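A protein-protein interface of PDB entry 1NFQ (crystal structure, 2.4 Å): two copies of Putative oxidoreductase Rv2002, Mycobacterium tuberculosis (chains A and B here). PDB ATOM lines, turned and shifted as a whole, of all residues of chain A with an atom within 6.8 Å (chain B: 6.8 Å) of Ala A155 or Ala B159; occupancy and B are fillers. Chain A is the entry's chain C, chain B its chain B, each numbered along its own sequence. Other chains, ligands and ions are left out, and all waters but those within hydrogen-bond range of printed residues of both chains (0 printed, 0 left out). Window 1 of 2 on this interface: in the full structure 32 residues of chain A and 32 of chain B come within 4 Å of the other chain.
ND1 of His A151 sits at hydrogen-bond distance from OG of Ser B166, 2.8 Å away.
O of Cys A150 sits at hydrogen-bond distance from OG1 of Thr A154 (2.8 Å).
O of Leu B163 lies within hydrogen-bond range of OG of Ser B166, at 3.3 Å.
Among the printed residues, pairs that only touch across the chains: Phe A158 with Phe B158, Ala A155 with Ala B159, Thr A154 with Gly B162, Ala A159 with Ala B155, Phe A158 with Gly B162, Trp A105 with Leu B113 and His A151 with Leu B163.
Printed residues of chain B within 4 Å of Trp A105: Leu B113 (3.8 Å).
Ala A155 touches just one residue of chain B: Ala B159 (3.4 Å).
Lys A157 touches none of the printed residues of chain B.
Printed residues of chain A within 4 Å of Ala B159: Ala A155.
Of the printed residues of chain A, Leu B163 touches His A151 (3.8 Å).
The nearest printed residue of chain B that does not touch Phe A158 is Arg B161 (4.1 Å).
Of the 17 printed residues of chain B, 7 touch a printed residue of chain A.
Hydrophobic or aromatic side chains of chain B within 4 Å of the printed part of chain A: Leu B113, Phe B158, Ala B159 and Leu B163.
Among the printed residues, 8 pairs touch across the chains.
Among the printed residues, no Asp or Glu carboxylate lies within 4 Å of a Lys or Arg side-chain nitrogen of the other chain.
Ala A155 touches Ala B159, and with the chains exchanged Ala A159 touches Ala B155.
Phe B158 touches its own counterpart, Phe A158.
Positions printed for both chains: 113, 153, 154, 155, 156, 157, 158, 159 and 160.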
ATOM      1  N   TRP A 105      -4.512   6.261 -16.582  1.00  0.00           N
ATOM      2  CA  TRP A 105      -3.650   5.983 -17.718  1.00  0.00           C
ATOM      3  C   TRP A 105      -4.270   6.558 -18.994  1.00  0.00           C
ATOM      4  O   TRP A 105      -3.590   7.235 -19.764  1.00  0.00           O
ATOM      5  CB  TRP A 105      -3.442   4.467 -17.851  1.00  0.00           C
ATOM      6  CG  TRP A 105      -2.880   4.014 -19.177  1.00  0.00           C
ATOM      7  CD1 TRP A 105      -3.588   3.594 -20.265  1.00  0.00           C
ATOM      8  CD2 TRP A 105      -1.494   3.944 -19.549  1.00  0.00           C
ATOM      9  NE1 TRP A 105      -2.731   3.264 -21.293  1.00  0.00           N
ATOM     10  CE2 TRP A 105      -1.442   3.470 -20.881  1.00  0.00           C
ATOM     11  CE3 TRP A 105      -0.293   4.239 -18.887  1.00  0.00           C
ATOM     12  CZ2 TRP A 105      -0.234   3.280 -21.564  1.00  0.00           C
ATOM     13  CZ3 TRP A 105       0.912   4.049 -19.569  1.00  0.00           C
ATOM     14  CH2 TRP A 105       0.929   3.574 -20.894  1.00  0.00           C
ATOM     15  N   LEU A 109      -3.116   9.948 -21.351  1.00  0.00           N
ATOM     16  CA  LEU A 109      -2.841   9.722 -22.770  1.00  0.00           C
ATOM     17  C   LEU A 109      -3.642  10.730 -23.601  1.00  0.00           C
ATOM     18  O   LEU A 109      -3.134  11.298 -24.575  1.00  0.00           O
ATOM     19  CB  LEU A 109      -3.239   8.305 -23.185  1.00  0.00           C
ATOM     20  CG  LEU A 109      -2.119   7.301 -23.474  1.00  0.00           C
ATOM     21  CD1 LEU A 109      -1.287   7.075 -22.229  1.00  0.00           C
ATOM     22  CD2 LEU A 109      -2.724   5.988 -23.937  1.00  0.00           C
ATOM     23  N   LEU A 113      -0.874  13.420 -24.758  1.00  0.00           N
ATOM     24  CA  LEU A 113      -0.472  12.946 -26.075  1.00  0.00           C
ATOM     25  C   LEU A 113      -1.463  13.292 -27.185  1.00  0.00           C
ATOM     26  O   LEU A 113      -1.113  13.992 -28.133  1.00  0.00           O
ATOM     27  CB  LEU A 113      -0.232  11.430 -26.033  1.00  0.00           C
ATOM     28  CG  LEU A 113       0.147  10.727 -27.344  1.00  0.00           C
ATOM     29  CD1 LEU A 113       1.295  11.469 -28.024  1.00  0.00           C
ATOM     30  CD2 LEU A 113       0.537   9.292 -27.048  1.00  0.00           C
ATOM     31  N   GLU A 142      11.488  13.792 -18.416  1.00  0.00           N
ATOM     32  CA  GLU A 142      10.872  12.489 -18.178  1.00  0.00           C
ATOM     33  C   GLU A 142      10.582  11.870 -19.538  1.00  0.00           C
ATOM     34  O   GLU A 142      10.114  10.738 -19.631  1.00  0.00           O
ATOM     35  CB  GLU A 142       9.569  12.597 -17.381  1.00  0.00           C
ATOM     36  CG  GLU A 142       9.760  12.797 -15.892  1.00  0.00           C
ATOM     37  CD  GLU A 142       9.926  14.256 -15.515  1.00  0.00           C
ATOM     38  OE1 GLU A 142      10.220  14.524 -14.333  1.00  0.00           O
ATOM     39  OE2 GLU A 142       9.753  15.135 -16.394  1.00  0.00           O
ATOM     40  N   CYS A 150       5.932   6.571 -12.492  1.00  0.00           N
ATOM     41  CA  CYS A 150       5.611   7.682 -13.379  1.00  0.00           C
ATOM     42  C   CYS A 150       5.414   7.171 -14.810  1.00  0.00           C
ATOM     43  O   CYS A 150       5.847   7.797 -15.778  1.00  0.00           O
ATOM     44  CB  CYS A 150       6.773   8.672 -13.330  1.00  0.00           C
ATOM     45  SG  CYS A 150       6.295  10.367 -13.417  1.00  0.00           S
ATOM     46  N   HIS A 151       4.734   6.041 -14.930  1.00  0.00           N
ATOM     47  CA  HIS A 151       4.518   5.386 -16.210  1.00  0.00           C
ATOM     48  C   HIS A 151       3.694   6.126 -17.257  1.00  0.00           C
ATOM     49  O   HIS A 151       4.089   6.188 -18.420  1.00  0.00           O
ATOM     50  CB  HIS A 151       3.956   3.991 -15.932  1.00  0.00           C
ATOM     51  CG  HIS A 151       4.706   3.276 -14.854  1.00  0.00           C
ATOM     52  ND1 HIS A 151       6.044   2.965 -14.965  1.00  0.00           N
ATOM     53  CD2 HIS A 151       4.344   2.927 -13.598  1.00  0.00           C
ATOM     54  CE1 HIS A 151       6.475   2.462 -13.823  1.00  0.00           C
ATOM     55  NE2 HIS A 151       5.462   2.430 -12.976  1.00  0.00           N
ATOM     56  N   GLY A 152       2.560   6.685 -16.862  1.00  0.00           N
ATOM     57  CA  GLY A 152       1.744   7.411 -17.817  1.00  0.00           C
ATOM     58  C   GLY A 152       2.444   8.674 -18.293  1.00  0.00           C
ATOM     59  O   GLY A 152       2.499   8.960 -19.489  1.00  0.00           O
ATOM     60  N   TYR A 153       2.997   9.428 -17.348  1.00  0.00           N
ATOM     61  CA  TYR A 153       3.689  10.666 -17.658  1.00  0.00           C
ATOM     62  C   TYR A 153       4.909  10.416 -18.552  1.00  0.00           C
ATOM     63  O   TYR A 153       5.099  11.100 -19.560  1.00  0.00           O
ATOM     64  CB  TYR A 153       4.121  11.349 -16.360  1.00  0.00           C
ATOM     65  CG  TYR A 153       4.553  12.790 -16.520  1.00  0.00           C
ATOM     66  CD1 TYR A 153       3.630  13.785 -16.844  1.00  0.00           C
ATOM     67  CD2 TYR A 153       5.879  13.164 -16.315  1.00  0.00           C
ATOM     68  CE1 TYR A 153       4.016  15.116 -16.953  1.00  0.00           C
ATOM     69  CE2 TYR A 153       6.278  14.494 -16.421  1.00  0.00           C
ATOM     70  CZ  TYR A 153       5.341  15.465 -16.735  1.00  0.00           C
ATOM     71  OH  TYR A 153       5.724  16.790 -16.812  1.00  0.00           O
ATOM     72  N   THR A 154       5.728   9.433 -18.181  1.00  0.00           N
ATOM     73  CA  THR A 154       6.922   9.096 -18.949  1.00  0.00           C
ATOM     74  C   THR A 154       6.560   8.656 -20.363  1.00  0.00           C
ATOM     75  O   THR A 154       7.163   9.101 -21.332  1.00  0.00           O
ATOM     76  CB  THR A 154       7.728   7.956 -18.270  1.00  0.00           C
ATOM     77  OG1 THR A 154       8.267   8.423 -17.032  1.00  0.00           O
ATOM     78  CG2 THR A 154       8.875   7.495 -19.158  1.00  0.00           C
ATOM     79  N   ALA A 155       5.571   7.778 -20.475  1.00  0.00           N
ATOM     80  CA  ALA A 155       5.158   7.282 -21.777  1.00  0.00           C
ATOM     81  C   ALA A 155       4.704   8.411 -22.704  1.00  0.00           C
ATOM     82  O   ALA A 155       5.119   8.474 -23.868  1.00  0.00           O
ATOM     83  CB  ALA A 155       4.050   6.252 -21.614  1.00  0.00           C
ATOM     84  N   THR A 156       3.865   9.311 -22.197  1.00  0.00           N
ATOM     85  CA  THR A 156       3.373  10.414 -23.019  1.00  0.00           C
ATOM     86  C   THR A 156       4.453  11.448 -23.372  1.00  0.00           C
ATOM     87  O   THR A 156       4.462  11.993 -24.480  1.00  0.00           O
ATOM     88  CB  THR A 156       2.172  11.143 -22.351  1.00  0.00           C
ATOM     89  OG1 THR A 156       2.566  11.686 -21.084  1.00  0.00           O
ATOM     90  CG2 THR A 156       1.010  10.177 -22.152  1.00  0.00           C
ATOM     91  N   LYS A 157       5.362  11.723 -22.445  1.00  0.00           N
ATOM     92  CA  LYS A 157       6.417  12.690 -22.720  1.00  0.00           C
ATOM     93  C   LYS A 157       7.413  12.148 -23.749  1.00  0.00           C
ATOM     94  O   LYS A 157       8.006  12.912 -24.508  1.00  0.00           O
ATOM     95  CB  LYS A 157       7.123  13.101 -21.426  1.00  0.00           C
ATOM     96  CG  LYS A 157       6.247  13.955 -20.521  1.00  0.00           C
ATOM     97  CD  LYS A 157       5.678  15.153 -21.281  1.00  0.00           C
ATOM     98  CE  LYS A 157       4.824  16.044 -20.383  1.00  0.00           C
ATOM     99  NZ  LYS A 157       4.331  17.264 -21.100  1.00  0.00           N
ATOM    100  N   PHE A 158       7.584  10.829 -23.779  1.00  0.00           N
ATOM    101  CA  PHE A 158       8.463  10.193 -24.753  1.00  0.00           C
ATOM    102  C   PHE A 158       7.745  10.236 -26.097  1.00  0.00           C
ATOM    103  O   PHE A 158       8.356  10.477 -27.136  1.00  0.00           O
ATOM    104  CB  PHE A 158       8.734   8.726 -24.378  1.00  0.00           C
ATOM    105  CG  PHE A 158      10.092   8.490 -23.763  1.00  0.00           C
ATOM    106  CD1 PHE A 158      10.331   8.777 -22.421  1.00  0.00           C
ATOM    107  CD2 PHE A 158      11.135   7.977 -24.532  1.00  0.00           C
ATOM    108  CE1 PHE A 158      11.594   8.558 -21.855  1.00  0.00           C
ATOM    109  CE2 PHE A 158      12.408   7.755 -23.976  1.00  0.00           C
ATOM    110  CZ  PHE A 158      12.631   8.046 -22.634  1.00  0.00           C
ATOM    111  N   ALA A 159       6.435  10.005 -26.066  1.00  0.00           N
ATOM    112  CA  ALA A 159       5.622  10.008 -27.278  1.00  0.00           C
ATOM    113  C   ALA A 159       5.613  11.385 -27.936  1.00  0.00           C
ATOM    114  O   ALA A 159       5.725  11.494 -29.158  1.00  0.00           O
ATOM    115  CB  ALA A 159       4.195   9.571 -26.949  1.00  0.00           C
ATOM    116  N   VAL A 160       5.468  12.430 -27.125  1.00  0.00           N
ATOM    117  CA  VAL A 160       5.449  13.799 -27.634  1.00  0.00           C
ATOM    118  C   VAL A 160       6.782  14.102 -28.310  1.00  0.00           C
ATOM    119  O   VAL A 160       6.839  14.814 -29.311  1.00  0.00           O
ATOM    120  CB  VAL A 160       5.205  14.809 -26.490  1.00  0.00           C
ATOM    121  CG1 VAL A 160       5.517  16.227 -26.956  1.00  0.00           C
ATOM    122  CG2 VAL A 160       3.763  14.720 -26.039  1.00  0.00           C
ATOM    123  N   ASN B 112      -0.546  -0.828 -29.683  1.00  0.00           N
ATOM    124  CA  ASN B 112       0.893  -0.620 -29.529  1.00  0.00           C
ATOM    125  C   ASN B 112       1.395  -0.063 -28.215  1.00  0.00           C
ATOM    126  O   ASN B 112       2.519  -0.353 -27.825  1.00  0.00           O
ATOM    127  CB  ASN B 112       1.412   0.259 -30.670  1.00  0.00           C
ATOM    128  CG  ASN B 112       1.402  -0.461 -32.009  1.00  0.00           C
ATOM    129  OD1 ASN B 112       0.707  -1.459 -32.187  1.00  0.00           O
ATOM    130  ND2 ASN B 112       2.164   0.055 -32.962  1.00  0.00           N
ATOM    131  N   LEU B 113       0.575   0.731 -27.536  1.00  0.00           N
ATOM    132  CA  LEU B 113       0.978   1.322 -26.272  1.00  0.00           C
ATOM    133  C   LEU B 113       0.239   0.749 -25.059  1.00  0.00           C
ATOM    134  O   LEU B 113       0.867   0.177 -24.167  1.00  0.00           O
ATOM    135  CB  LEU B 113       0.801   2.843 -26.329  1.00  0.00           C
ATOM    136  CG  LEU B 113       1.137   3.638 -25.063  1.00  0.00           C
ATOM    137  CD1 LEU B 113       2.497   3.221 -24.516  1.00  0.00           C
ATOM    138  CD2 LEU B 113       1.116   5.121 -25.387  1.00  0.00           C
ATOM    139  N   SER B 139       9.927  -2.471 -29.613  1.00  0.00           N
ATOM    140  CA  SER B 139       9.717  -1.130 -30.144  1.00  0.00           C
ATOM    141  C   SER B 139      10.173  -1.228 -31.612  1.00  0.00           C
ATOM    142  O   SER B 139       9.825  -2.186 -32.303  1.00  0.00           O
ATOM    143  CB  SER B 139      10.574  -0.129 -29.366  1.00  0.00           C
ATOM    144  OG  SER B 139      10.376   1.191 -29.832  1.00  0.00           O
ATOM    145  N   GLY B 143      11.130   4.278 -33.055  1.00  0.00           N
ATOM    146  CA  GLY B 143      11.002   4.719 -31.680  1.00  0.00           C
ATOM    147  C   GLY B 143      12.282   5.458 -31.302  1.00  0.00           C
ATOM    148  O   GLY B 143      12.499   5.799 -30.134  1.00  0.00           O
ATOM    149  N   TYR B 153       2.372   5.413 -35.250  1.00  0.00           N
ATOM    150  CA  TYR B 153       3.383   4.387 -35.049  1.00  0.00           C
ATOM    151  C   TYR B 153       4.609   4.948 -34.319  1.00  0.00           C
ATOM    152  O   TYR B 153       5.096   4.348 -33.364  1.00  0.00           O
ATOM    153  CB  TYR B 153       3.792   3.804 -36.402  1.00  0.00           C
ATOM    154  CG  TYR B 153       4.581   2.522 -36.323  1.00  0.00           C
ATOM    155  CD1 TYR B 153       3.979   1.336 -35.898  1.00  0.00           C
ATOM    156  CD2 TYR B 153       5.926   2.485 -36.694  1.00  0.00           C
ATOM    157  CE1 TYR B 153       4.699   0.142 -35.847  1.00  0.00           C
ATOM    158  CE2 TYR B 153       6.656   1.299 -36.645  1.00  0.00           C
ATOM    159  CZ  TYR B 153       6.035   0.132 -36.224  1.00  0.00           C
ATOM    160  OH  TYR B 153       6.748  -1.038 -36.196  1.00  0.00           O
ATOM    161  N   THR B 154       5.101   6.098 -34.770  1.00  0.00           N
ATOM    162  CA  THR B 154       6.260   6.729 -34.148  1.00  0.00           C
ATOM    163  C   THR B 154       5.979   7.094 -32.691  1.00  0.00           C
ATOM    164  O   THR B 154       6.788   6.829 -31.807  1.00  0.00           O
ATOM    165  CB  THR B 154       6.680   8.020 -34.902  1.00  0.00           C
ATOM    166  OG1 THR B 154       7.174   7.675 -36.200  1.00  0.00           O
ATOM    167  CG2 THR B 154       7.769   8.767 -34.140  1.00  0.00           C
ATOM    168  N   ALA B 155       4.831   7.703 -32.445  1.00  0.00           N
ATOM    169  CA  ALA B 155       4.477   8.102 -31.094  1.00  0.00           C
ATOM    170  C   ALA B 155       4.430   6.910 -30.136  1.00  0.00           C
ATOM    171  O   ALA B 155       4.981   6.977 -29.037  1.00  0.00           O
ATOM    172  CB  ALA B 155       3.139   8.823 -31.103  1.00  0.00           C
ATOM    173  N   THR B 156       3.791   5.817 -30.550  1.00  0.00           N
ATOM    174  CA  THR B 156       3.683   4.650 -29.685  1.00  0.00           C
ATOM    175  C   THR B 156       5.011   3.925 -29.488  1.00  0.00           C
ATOM    176  O   THR B 156       5.289   3.425 -28.400  1.00  0.00           O
ATOM    177  CB  THR B 156       2.618   3.634 -30.203  1.00  0.00           C
ATOM    178  OG1 THR B 156       2.979   3.158 -31.506  1.00  0.00           O
ATOM    179  CG2 THR B 156       1.236   4.290 -30.257  1.00  0.00           C
ATOM    180  N   LYS B 157       5.839   3.865 -30.528  1.00  0.00           N
ATOM    181  CA  LYS B 157       7.122   3.186 -30.399  1.00  0.00           C
ATOM    182  C   LYS B 157       8.072   3.970 -29.495  1.00  0.00           C
ATOM    183  O   LYS B 157       8.912   3.382 -28.829  1.00  0.00           O
ATOM    184  CB  LYS B 157       7.741   2.939 -31.776  1.00  0.00           C
ATOM    185  CG  LYS B 157       6.998   1.879 -32.572  1.00  0.00           C
ATOM    186  CD  LYS B 157       6.833   0.594 -31.755  1.00  0.00           C
ATOM    187  CE  LYS B 157       6.135  -0.501 -32.550  1.00  0.00           C
ATOM    188  NZ  LYS B 157       6.062  -1.796 -31.803  1.00  0.00           N
ATOM    189  N   PHE B 158       7.930   5.294 -29.474  1.00  0.00           N
ATOM    190  CA  PHE B 158       8.743   6.140 -28.602  1.00  0.00           C
ATOM    191  C   PHE B 158       8.232   5.944 -27.165  1.00  0.00           C
ATOM    192  O   PHE B 158       9.009   5.881 -26.216  1.00  0.00           O
ATOM    193  CB  PHE B 158       8.595   7.627 -28.979  1.00  0.00           C
ATOM    194  CG  PHE B 158       9.762   8.183 -29.764  1.00  0.00           C
ATOM    195  CD1 PHE B 158       9.887   7.945 -31.134  1.00  0.00           C
ATOM    196  CD2 PHE B 158      10.741   8.940 -29.126  1.00  0.00           C
ATOM    197  CE1 PHE B 158      10.978   8.455 -31.851  1.00  0.00           C
ATOM    198  CE2 PHE B 158      11.831   9.452 -29.832  1.00  0.00           C
ATOM    199  CZ  PHE B 158      11.951   9.211 -31.194  1.00  0.00           C
ATOM    200  N   ALA B 159       6.914   5.841 -27.027  1.00  0.00           N
ATOM    201  CA  ALA B 159       6.284   5.664 -25.728  1.00  0.00           C
ATOM    202  C   ALA B 159       6.695   4.343 -25.092  1.00  0.00           C
ATOM    203  O   ALA B 159       6.980   4.287 -23.891  1.00  0.00           O
ATOM    204  CB  ALA B 159       4.761   5.734 -25.870  1.00  0.00           C
ATOM    205  N   VAL B 160       6.725   3.285 -25.900  1.00  0.00           N
ATOM    206  CA  VAL B 160       7.096   1.958 -25.419  1.00  0.00           C
ATOM    207  C   VAL B 160       8.527   1.994 -24.918  1.00  0.00           C
ATOM    208  O   VAL B 160       8.872   1.338 -23.941  1.00  0.00           O
ATOM    209  CB  VAL B 160       6.959   0.899 -26.537  1.00  0.00           C
ATOM    210  CG1 VAL B 160       7.657  -0.391 -26.132  1.00  0.00           C
ATOM    211  CG2 VAL B 160       5.490   0.629 -26.805  1.00  0.00           C
ATOM    212  N   ARG B 161       9.353   2.773 -25.601  1.00  0.00           N
ATOM    213  CA  ARG B 161      10.751   2.945 -25.233  1.00  0.00           C
ATOM    214  C   ARG B 161      10.833   3.607 -23.846  1.00  0.00           C
ATOM    215  O   ARG B 161      11.642   3.213 -23.002  1.00  0.00           O
ATOM    216  CB  ARG B 161      11.423   3.820 -26.286  1.00  0.00           C
ATOM    217  CG  ARG B 161      12.843   4.242 -26.001  1.00  0.00           C
ATOM    218  CD  ARG B 161      13.258   5.264 -27.061  1.00  0.00           C
ATOM    219  NE  ARG B 161      14.602   5.789 -26.858  1.00  0.00           N
ATOM    220  CZ  ARG B 161      15.090   6.838 -27.510  1.00  0.00           C
ATOM    221  NH1 ARG B 161      14.342   7.471 -28.412  1.00  0.00           N
ATOM    222  NH2 ARG B 161      16.319   7.270 -27.243  1.00  0.00           N
ATOM    223  N   GLY B 162       9.983   4.605 -23.619  1.00  0.00           N
ATOM    224  CA  GLY B 162       9.971   5.292 -22.342  1.00  0.00           C
ATOM    225  C   GLY B 162       9.384   4.435 -21.235  1.00  0.00           C
ATOM    226  O   GLY B 162       9.915   4.391 -20.122  1.00  0.00           O
ATOM    227  N   LEU B 163       8.286   3.751 -21.539  1.00  0.00           N
ATOM    228  CA  LEU B 163       7.618   2.893 -20.568  1.00  0.00           C
ATOM    229  C   LEU B 163       8.589   1.818 -20.079  1.00  0.00           C
ATOM    230  O   LEU B 163       8.524   1.387 -18.925  1.00  0.00           O
ATOM    231  CB  LEU B 163       6.381   2.248 -21.206  1.00  0.00           C
ATOM    232  CG  LEU B 163       5.483   1.402 -20.302  1.00  0.00           C
ATOM    233  CD1 LEU B 163       4.932   2.259 -19.168  1.00  0.00           C
ATOM    234  CD2 LEU B 163       4.359   0.812 -21.124  1.00  0.00           C
ATOM    235  N   THR B 164       9.491   1.399 -20.964  1.00  0.00           N
ATOM    236  CA  THR B 164      10.496   0.386 -20.648  1.00  0.00           C
ATOM    237  C   THR B 164      11.409   0.859 -19.516  1.00  0.00           C
ATOM    238  O   THR B 164      11.755   0.084 -18.622  1.00  0.00           O
ATOM    239  CB  THR B 164      11.377   0.066 -21.892  1.00  0.00           C
ATOM    240  OG1 THR B 164      10.580  -0.574 -22.889  1.00  0.00           O
ATOM    241  CG2 THR B 164      12.526  -0.848 -21.527  1.00  0.00           C
ATOM    242  N   SER B 166      10.834   3.479 -17.158  1.00  0.00           N
ATOM    243  CA  SER B 166      10.168   3.720 -15.891  1.00  0.00           C
ATOM    244  C   SER B 166       9.840   2.404 -15.178  1.00  0.00           C
ATOM    245  O   SER B 166      10.017   2.293 -13.968  1.00  0.00           O
ATOM    246  CB  SER B 166       8.896   4.560 -16.098  1.00  0.00           C
ATOM    247  OG  SER B 166       7.920   3.859 -16.844  1.00  0.00           O
